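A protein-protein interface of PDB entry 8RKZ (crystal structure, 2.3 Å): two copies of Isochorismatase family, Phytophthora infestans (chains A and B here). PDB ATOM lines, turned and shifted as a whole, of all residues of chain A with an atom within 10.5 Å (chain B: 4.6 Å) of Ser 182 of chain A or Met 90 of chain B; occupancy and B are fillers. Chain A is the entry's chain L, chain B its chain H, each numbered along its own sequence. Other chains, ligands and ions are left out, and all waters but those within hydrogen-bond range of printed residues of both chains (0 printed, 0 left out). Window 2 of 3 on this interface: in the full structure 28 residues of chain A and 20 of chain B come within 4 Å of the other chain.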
ATOM      1  N   PHE A 175      33.275   9.527 -13.457  1.00  0.00           N
ATOM      2  CA  PHE A 175      31.930  10.026 -13.179  1.00  0.00           C
ATOM      3  C   PHE A 175      31.961  11.219 -12.233  1.00  0.00           C
ATOM      4  O   PHE A 175      31.096  12.099 -12.317  1.00  0.00           O
ATOM      5  CB  PHE A 175      31.049   8.916 -12.603  1.00  0.00           C
ATOM      6  CG  PHE A 175      30.382   8.072 -13.652  1.00  0.00           C
ATOM      7  CD1 PHE A 175      29.289   8.551 -14.355  1.00  0.00           C
ATOM      8  CD2 PHE A 175      30.845   6.795 -13.931  1.00  0.00           C
ATOM      9  CE1 PHE A 175      28.677   7.777 -15.325  1.00  0.00           C
ATOM     10  CE2 PHE A 175      30.234   6.011 -14.899  1.00  0.00           C
ATOM     11  CZ  PHE A 175      29.151   6.503 -15.597  1.00  0.00           C
ATOM     12  N   LEU A 177      34.316  13.552 -12.303  1.00  0.00           N
ATOM     13  CA  LEU A 177      34.635  14.686 -13.163  1.00  0.00           C
ATOM     14  C   LEU A 177      33.430  15.112 -13.996  1.00  0.00           C
ATOM     15  O   LEU A 177      33.205  16.311 -14.198  1.00  0.00           O
ATOM     16  CB  LEU A 177      35.824  14.344 -14.058  1.00  0.00           C
ATOM     17  CG  LEU A 177      37.153  14.185 -13.314  1.00  0.00           C
ATOM     18  CD1 LEU A 177      38.124  13.311 -14.091  1.00  0.00           C
ATOM     19  CD2 LEU A 177      37.762  15.552 -13.024  1.00  0.00           C
ATOM     20  N   ALA A 178      32.643  14.148 -14.480  1.00  0.00           N
ATOM     21  CA  ALA A 178      31.492  14.475 -15.318  1.00  0.00           C
ATOM     22  C   ALA A 178      30.417  15.217 -14.527  1.00  0.00           C
ATOM     23  O   ALA A 178      29.901  16.247 -14.978  1.00  0.00           O
ATOM     24  CB  ALA A 178      30.925  13.197 -15.937  1.00  0.00           C
ATOM     25  N   ASN A 179      30.036  14.672 -13.369  1.00  0.00           N
ATOM     26  CA  ASN A 179      29.252  15.332 -12.323  1.00  0.00           C
ATOM     27  C   ASN A 179      27.778  15.511 -12.680  1.00  0.00           C
ATOM     28  O   ASN A 179      26.946  15.716 -11.789  1.00  0.00           O
ATOM     29  CB  ASN A 179      29.889  16.696 -11.990  1.00  0.00           C
ATOM     30  CG  ASN A 179      28.900  17.690 -11.380  1.00  0.00           C
ATOM     31  OD1 ASN A 179      28.570  17.603 -10.196  1.00  0.00           O
ATOM     32  ND2 ASN A 179      28.424  18.633 -12.187  1.00  0.00           N
ATOM     33  N   ASP A 180      27.417  15.327 -13.949  1.00  0.00           N
ATOM     34  CA  ASP A 180      26.044  15.567 -14.385  1.00  0.00           C
ATOM     35  C   ASP A 180      25.825  15.028 -15.790  1.00  0.00           C
ATOM     36  O   ASP A 180      26.562  15.376 -16.719  1.00  0.00           O
ATOM     37  CB  ASP A 180      25.705  17.064 -14.335  1.00  0.00           C
ATOM     38  CG  ASP A 180      24.206  17.340 -14.456  1.00  0.00           C
ATOM     39  OD1 ASP A 180      23.510  16.613 -15.195  1.00  0.00           O
ATOM     40  OD2 ASP A 180      23.718  18.296 -13.820  1.00  0.00           O
ATOM     41  N   ALA A 181      24.791  14.202 -15.960  1.00  0.00           N
ATOM     42  CA  ALA A 181      24.536  13.605 -17.262  1.00  0.00           C
ATOM     43  C   ALA A 181      24.005  14.619 -18.264  1.00  0.00           C
ATOM     44  O   ALA A 181      24.043  14.356 -19.469  1.00  0.00           O
ATOM     45  CB  ALA A 181      23.559  12.437 -17.119  1.00  0.00           C
ATOM     46  N   SER A 182      23.518  15.769 -17.794  1.00  0.00           N
ATOM     47  CA  SER A 182      23.019  16.811 -18.683  1.00  0.00           C
ATOM     48  C   SER A 182      24.131  17.646 -19.310  1.00  0.00           C
ATOM     49  O   SER A 182      23.854  18.409 -20.242  1.00  0.00           O
ATOM     50  CB  SER A 182      22.049  17.720 -17.925  1.00  0.00           C
ATOM     51  OG  SER A 182      22.736  18.777 -17.280  1.00  0.00           O
ATOM     52  N   ASN A 183      25.368  17.520 -18.835  1.00  0.00           N
ATOM     53  CA  ASN A 183      26.475  18.239 -19.445  1.00  0.00           C
ATOM     54  C   ASN A 183      26.663  17.774 -20.889  1.00  0.00           C
ATOM     55  O   ASN A 183      26.407  16.611 -21.214  1.00  0.00           O
ATOM     56  CB  ASN A 183      27.760  18.027 -18.644  1.00  0.00           C
ATOM     57  CG  ASN A 183      27.710  18.685 -17.277  1.00  0.00           C
ATOM     58  OD1 ASN A 183      26.695  19.270 -16.895  1.00  0.00           O
ATOM     59  ND2 ASN A 183      28.801  18.582 -16.528  1.00  0.00           N
ATOM     60  N   PRO A 184      27.101  18.670 -21.782  1.00  0.00           N
ATOM     61  CA  PRO A 184      27.207  18.302 -23.202  1.00  0.00           C
ATOM     62  C   PRO A 184      28.292  17.282 -23.503  1.00  0.00           C
ATOM     63  O   PRO A 184      28.276  16.709 -24.596  1.00  0.00           O
ATOM     64  CB  PRO A 184      27.500  19.643 -23.882  1.00  0.00           C
ATOM     65  CG  PRO A 184      28.247  20.410 -22.847  1.00  0.00           C
ATOM     66  CD  PRO A 184      27.638  20.018 -21.522  1.00  0.00           C
ATOM     67  N   GLU A 185      29.228  17.035 -22.591  1.00  0.00           N
ATOM     68  CA  GLU A 185      30.277  16.050 -22.819  1.00  0.00           C
ATOM     69  C   GLU A 185      29.876  14.642 -22.413  1.00  0.00           C
ATOM     70  O   GLU A 185      30.642  13.704 -22.659  1.00  0.00           O
ATOM     71  CB  GLU A 185      31.549  16.430 -22.050  1.00  0.00           C
ATOM     72  CG  GLU A 185      32.228  17.681 -22.554  1.00  0.00           C
ATOM     73  CD  GLU A 185      31.809  18.911 -21.779  1.00  0.00           C
ATOM     74  OE1 GLU A 185      30.724  18.881 -21.157  1.00  0.00           O
ATOM     75  OE2 GLU A 185      32.564  19.907 -21.797  1.00  0.00           O
ATOM     76  N   PHE A 186      28.710  14.467 -21.790  1.00  0.00           N
ATOM     77  CA  PHE A 186      28.389  13.161 -21.228  1.00  0.00           C
ATOM     78  C   PHE A 186      28.129  12.114 -22.304  1.00  0.00           C
ATOM     79  O   PHE A 186      28.354  10.922 -22.064  1.00  0.00           O
ATOM     80  CB  PHE A 186      27.185  13.254 -20.298  1.00  0.00           C
ATOM     81  CG  PHE A 186      26.928  11.992 -19.549  1.00  0.00           C
ATOM     82  CD1 PHE A 186      27.883  11.486 -18.684  1.00  0.00           C
ATOM     83  CD2 PHE A 186      25.758  11.280 -19.746  1.00  0.00           C
ATOM     84  CE1 PHE A 186      27.661  10.305 -18.002  1.00  0.00           C
ATOM     85  CE2 PHE A 186      25.529  10.097 -19.068  1.00  0.00           C
ATOM     86  CZ  PHE A 186      26.482   9.608 -18.194  1.00  0.00           C
ATOM     87  N   LYS A 187      27.664  12.527 -23.485  1.00  0.00           N
ATOM     88  CA  LYS A 187      27.361  11.548 -24.527  1.00  0.00           C
ATOM     89  C   LYS A 187      28.612  10.776 -24.936  1.00  0.00           C
ATOM     90  O   LYS A 187      28.567   9.552 -25.103  1.00  0.00           O
ATOM     91  CB  LYS A 187      26.699  12.227 -25.736  1.00  0.00           C
ATOM     92  CG  LYS A 187      27.605  13.013 -26.712  1.00  0.00           C
ATOM     93  CD  LYS A 187      28.472  14.065 -26.030  1.00  0.00           C
ATOM     94  CE  LYS A 187      29.365  14.810 -27.010  1.00  0.00           C
ATOM     95  NZ  LYS A 187      30.428  15.579 -26.291  1.00  0.00           N
ATOM     96  N   ILE A 188      29.743  11.462 -25.063  1.00  0.00           N
ATOM     97  CA  ILE A 188      30.956  10.794 -25.506  1.00  0.00           C
ATOM     98  C   ILE A 188      31.693  10.161 -24.331  1.00  0.00           C
ATOM     99  O   ILE A 188      32.403   9.167 -24.513  1.00  0.00           O
ATOM    100  CB  ILE A 188      31.849  11.776 -26.286  1.00  0.00           C
ATOM    101  CG1 ILE A 188      33.057  11.054 -26.879  1.00  0.00           C
ATOM    102  CG2 ILE A 188      32.293  12.928 -25.394  1.00  0.00           C
ATOM    103  CD1 ILE A 188      33.927  11.939 -27.738  1.00  0.00           C
ATOM    104  N   ILE A 189      31.518  10.703 -23.120  1.00  0.00           N
ATOM    105  CA  ILE A 189      32.050  10.048 -21.929  1.00  0.00           C
ATOM    106  C   ILE A 189      31.343   8.717 -21.697  1.00  0.00           C
ATOM    107  O   ILE A 189      31.972   7.727 -21.307  1.00  0.00           O
ATOM    108  CB  ILE A 189      31.936  10.979 -20.709  1.00  0.00           C
ATOM    109  CG1 ILE A 189      32.993  12.080 -20.779  1.00  0.00           C
ATOM    110  CG2 ILE A 189      32.101  10.206 -19.419  1.00  0.00           C
ATOM    111  CD1 ILE A 189      32.807  13.159 -19.739  1.00  0.00           C
ATOM    112  N   SER A 190      30.028   8.669 -21.947  1.00  0.00           N
ATOM    113  CA  SER A 190      29.298   7.407 -21.857  1.00  0.00           C
ATOM    114  C   SER A 190      29.870   6.373 -22.818  1.00  0.00           C
ATOM    115  O   SER A 190      30.046   5.203 -22.451  1.00  0.00           O
ATOM    116  CB  SER A 190      27.811   7.622 -22.152  1.00  0.00           C
ATOM    117  OG  SER A 190      27.242   8.620 -21.327  1.00  0.00           O
ATOM    118  N   GLN B  62      17.500   8.605 -11.613  1.00  0.00           N
ATOM    119  CA  GLN B  62      18.451   9.150 -12.577  1.00  0.00           C
ATOM    120  C   GLN B  62      17.892   8.919 -13.978  1.00  0.00           C
ATOM    121  O   GLN B  62      17.746   7.770 -14.408  1.00  0.00           O
ATOM    122  CB  GLN B  62      19.822   8.499 -12.405  1.00  0.00           C
ATOM    123  CG  GLN B  62      20.826   8.801 -13.510  1.00  0.00           C
ATOM    124  CD  GLN B  62      21.393  10.208 -13.432  1.00  0.00           C
ATOM    125  OE1 GLN B  62      21.372  10.843 -12.376  1.00  0.00           O
ATOM    126  NE2 GLN B  62      21.919  10.697 -14.549  1.00  0.00           N
ATOM    127  N   TYR B  63      17.569  10.009 -14.678  1.00  0.00           N
ATOM    128  CA  TYR B  63      17.080   9.966 -16.059  1.00  0.00           C
ATOM    129  C   TYR B  63      15.905   8.997 -16.188  1.00  0.00           C
ATOM    130  O   TYR B  63      15.928   8.041 -16.965  1.00  0.00           O
ATOM    131  CB  TYR B  63      18.218   9.600 -17.021  1.00  0.00           C
ATOM    132  CG  TYR B  63      18.026  10.056 -18.458  1.00  0.00           C
ATOM    133  CD1 TYR B  63      16.775  10.440 -18.934  1.00  0.00           C
ATOM    134  CD2 TYR B  63      19.099  10.097 -19.343  1.00  0.00           C
ATOM    135  CE1 TYR B  63      16.601  10.850 -20.245  1.00  0.00           C
ATOM    136  CE2 TYR B  63      18.934  10.506 -20.657  1.00  0.00           C
ATOM    137  CZ  TYR B  63      17.685  10.882 -21.102  1.00  0.00           C
ATOM    138  OH  TYR B  63      17.519  11.292 -22.408  1.00  0.00           O
ATOM    139  N   LYS B  89      16.380  13.455 -11.615  1.00  0.00           N
ATOM    140  CA  LYS B  89      17.603  14.231 -11.742  1.00  0.00           C
ATOM    141  C   LYS B  89      18.443  13.713 -12.900  1.00  0.00           C
ATOM    142  O   LYS B  89      18.291  12.577 -13.357  1.00  0.00           O
ATOM    143  CB  LYS B  89      18.433  14.186 -10.451  1.00  0.00           C
ATOM    144  CG  LYS B  89      19.077  12.832 -10.182  1.00  0.00           C
ATOM    145  CD  LYS B  89      19.713  12.784  -8.803  1.00  0.00           C
ATOM    146  CE  LYS B  89      20.191  11.385  -8.463  1.00  0.00           C
ATOM    147  NZ  LYS B  89      21.180  10.872  -9.448  1.00  0.00           N
ATOM    148  N   MET B  90      19.326  14.586 -13.377  1.00  0.00           N
ATOM    149  CA  MET B  90      20.416  14.201 -14.260  1.00  0.00           C
ATOM    150  C   MET B  90      21.771  14.290 -13.574  1.00  0.00           C
ATOM    151  O   MET B  90      22.681  13.535 -13.926  1.00  0.00           O
ATOM    152  CB  MET B  90      20.417  15.083 -15.515  1.00  0.00           C
ATOM    153  CG  MET B  90      19.252  14.810 -16.475  1.00  0.00           C
ATOM    154  SD  MET B  90      19.269  13.188 -17.277  1.00  0.00           S
ATOM    155  CE  MET B  90      20.410  13.498 -18.622  1.00  0.00           C
ATOM    156  N   LYS B  91      21.911  15.180 -12.594  1.00  0.00           N
ATOM    157  CA  LYS B  91      23.123  15.247 -11.789  1.00  0.00           C
ATOM    158  C   LYS B  91      23.284  13.972 -10.973  1.00  0.00           C
ATOM    159  O   LYS B  91      22.327  13.473 -10.377  1.00  0.00           O
ATOM    160  CB  LYS B  91      23.078  16.466 -10.865  1.00  0.00           C
ATOM    161  CG  LYS B  91      24.394  16.757 -10.166  1.00  0.00           C
ATOM    162  CD  LYS B  91      24.407  18.136  -9.525  1.00  0.00           C
ATOM    163  CE  LYS B  91      25.705  18.372  -8.761  1.00  0.00           C
ATOM    164  NZ  LYS B  91      25.484  19.142  -7.506  1.00  0.00           N
ATOM    165  N   PHE B  92      24.508  13.437 -10.955  1.00  0.00           N
ATOM    166  CA  PHE B  92      24.739  12.146 -10.315  1.00  0.00           C
ATOM    167  C   PHE B  92      24.483  12.220  -8.816  1.00  0.00           C
ATOM    168  O   PHE B  92      23.894  11.303  -8.232  1.00  0.00           O
ATOM    169  CB  PHE B  92      26.159  11.667 -10.611  1.00  0.00           C
ATOM    170  CG  PHE B  92      26.434  11.484 -12.075  1.00  0.00           C
ATOM    171  CD1 PHE B  92      25.571  10.747 -12.871  1.00  0.00           C
ATOM    172  CD2 PHE B  92      27.533  12.087 -12.666  1.00  0.00           C
ATOM    173  CE1 PHE B  92      25.816  10.585 -14.225  1.00  0.00           C
ATOM    174  CE2 PHE B  92      27.782  11.936 -14.019  1.00  0.00           C
ATOM    175  CZ  PHE B  92      26.920  11.183 -14.801  1.00  0.00           C
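Among the printed residues, merely in contact across the chains: Asn 179 of chain A with Lys 91 of chain B (3.2 Å), Phe 186 of chain A with Phe 92 of chain B (3.4 Å), Asp 180 of chain A with Phe 92 of chain B (3.4 Å), Ala 181 of chain A with Gln 62 of chain B (3.5 Å), Phe 175 of chain A with Phe 92 of chain B (3.6 Å), Ala 181 of chain A with Phe 92 of chain B (3.9 Å), Ala 178 of chain A with Phe 92 of chain B (3.9 Å) and Ser 182 of chain A with Met 90 of chain B (3.9 Å).
The backbone carbonyl oxygen of Met 90 of chain B lies within hydrogen-bond range of the backbone NH of Ala 181 of chain A (3.0 Å). The backbone carbonyl oxygen of Met 90 of chain B sits close to the side-chain carboxylate of Asp 180 of chain A (3.4 Å). The side-chain carboxylate of Asp 180 of chain A lies within hydrogen-bond range of the backbone NH of Lys 91 of chain B. N of Phe 92 of chain B is in hydrogen-bond range of O of Asn 179 of chain A (3.4 Å).
Of the 6 printed residues of chain B, 4 touch a printed residue of chain A. Hydrophobic or aromatic side chains of chain B within 4 Å of the printed part of chain A: Met 90 and Phe 92. Of the 15 printed residues of chain A, 7 touch a printed residue of chain B. Hydrophobic or aromatic side chains of chain A that line the printed part of chain B: Phe 175, Ala 178, Ala 181 and Phe 186. Among the printed residues, 12 pairs touch across the chains.
No position is printed for both chains. Of the 12 pairs that touch across the chains among the printed residues, none has its exchanged pair printed and touching as well.
Of the printed residues of chain B, Asn 179 of chain A touches Lys 91 (3.2 Å) and Phe 92 (3.4 Å). Of the printed residues of chain B, Asp 180 of chain A touches Met 90 (3.3 Å), Lys 91 (3.4 Å) and Phe 92 (3.4 Å). Pro 184 of chain A touches none of the printed residues of chain B. Ile 188 of chain A touches none of the printed residues of chain B. Of the printed residues of chain A, Gln 62 of chain B touches Ala 181 (3.5 Å). Lys 89 of chain B touches none of the printed residues of chain A. Of chain A, only Asp 180 (3.3 Å), Ala 181 (3.0 Å) and Ser 182 (3.9 Å) come within 4 Å of Met 90 of chain B. Phe 92 of chain B touches just these residues of chain A: Phe 175, Ala 178, Asn 179, Asp 180, Ala 181 and Phe 186. The nearest printed residue of chain B that does not touch Ser 182 of chain A is Lys 91 of chain B (5.5 Å). The nearest residue of chain A that does not touch Met 90 of chain B is Asn 179 of chain A (5.2 Å). The nearest printed residue of chain B that does not touch Ala 178 of chain A is Lys 91 of chain B (7.3 Å).
The side-chain amino group (NZ) of Lys 89 of chain B lies within hydrogen-bond range of the backbone carbonyl oxygen (O) of Phe 92 of chain B (3.0 Å). The side-chain amino group (NZ) of Lys 89 of chain B lies within hydrogen-bond range of the backbone carbonyl oxygen (O) of Lys 91 of chain B. The backbone carbonyl oxygen (O) of Met 90 of chain B lies within hydrogen-bond range of the side-chain amide nitrogen (NE2) of Gln 62 of chain B, at 3.0 Å. OE1 of Gln 62 of chain B sits close to O of Lys 91 of chain B (3.4 Å). NZ of Lys 89 of chain B lies within hydrogen-bond range of OE1 of Gln 62 of chain B (2.9 Å). O of Phe 186 of chain A is in hydrogen-bond range of OG of Ser 190 of chain A (2.7 Å).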
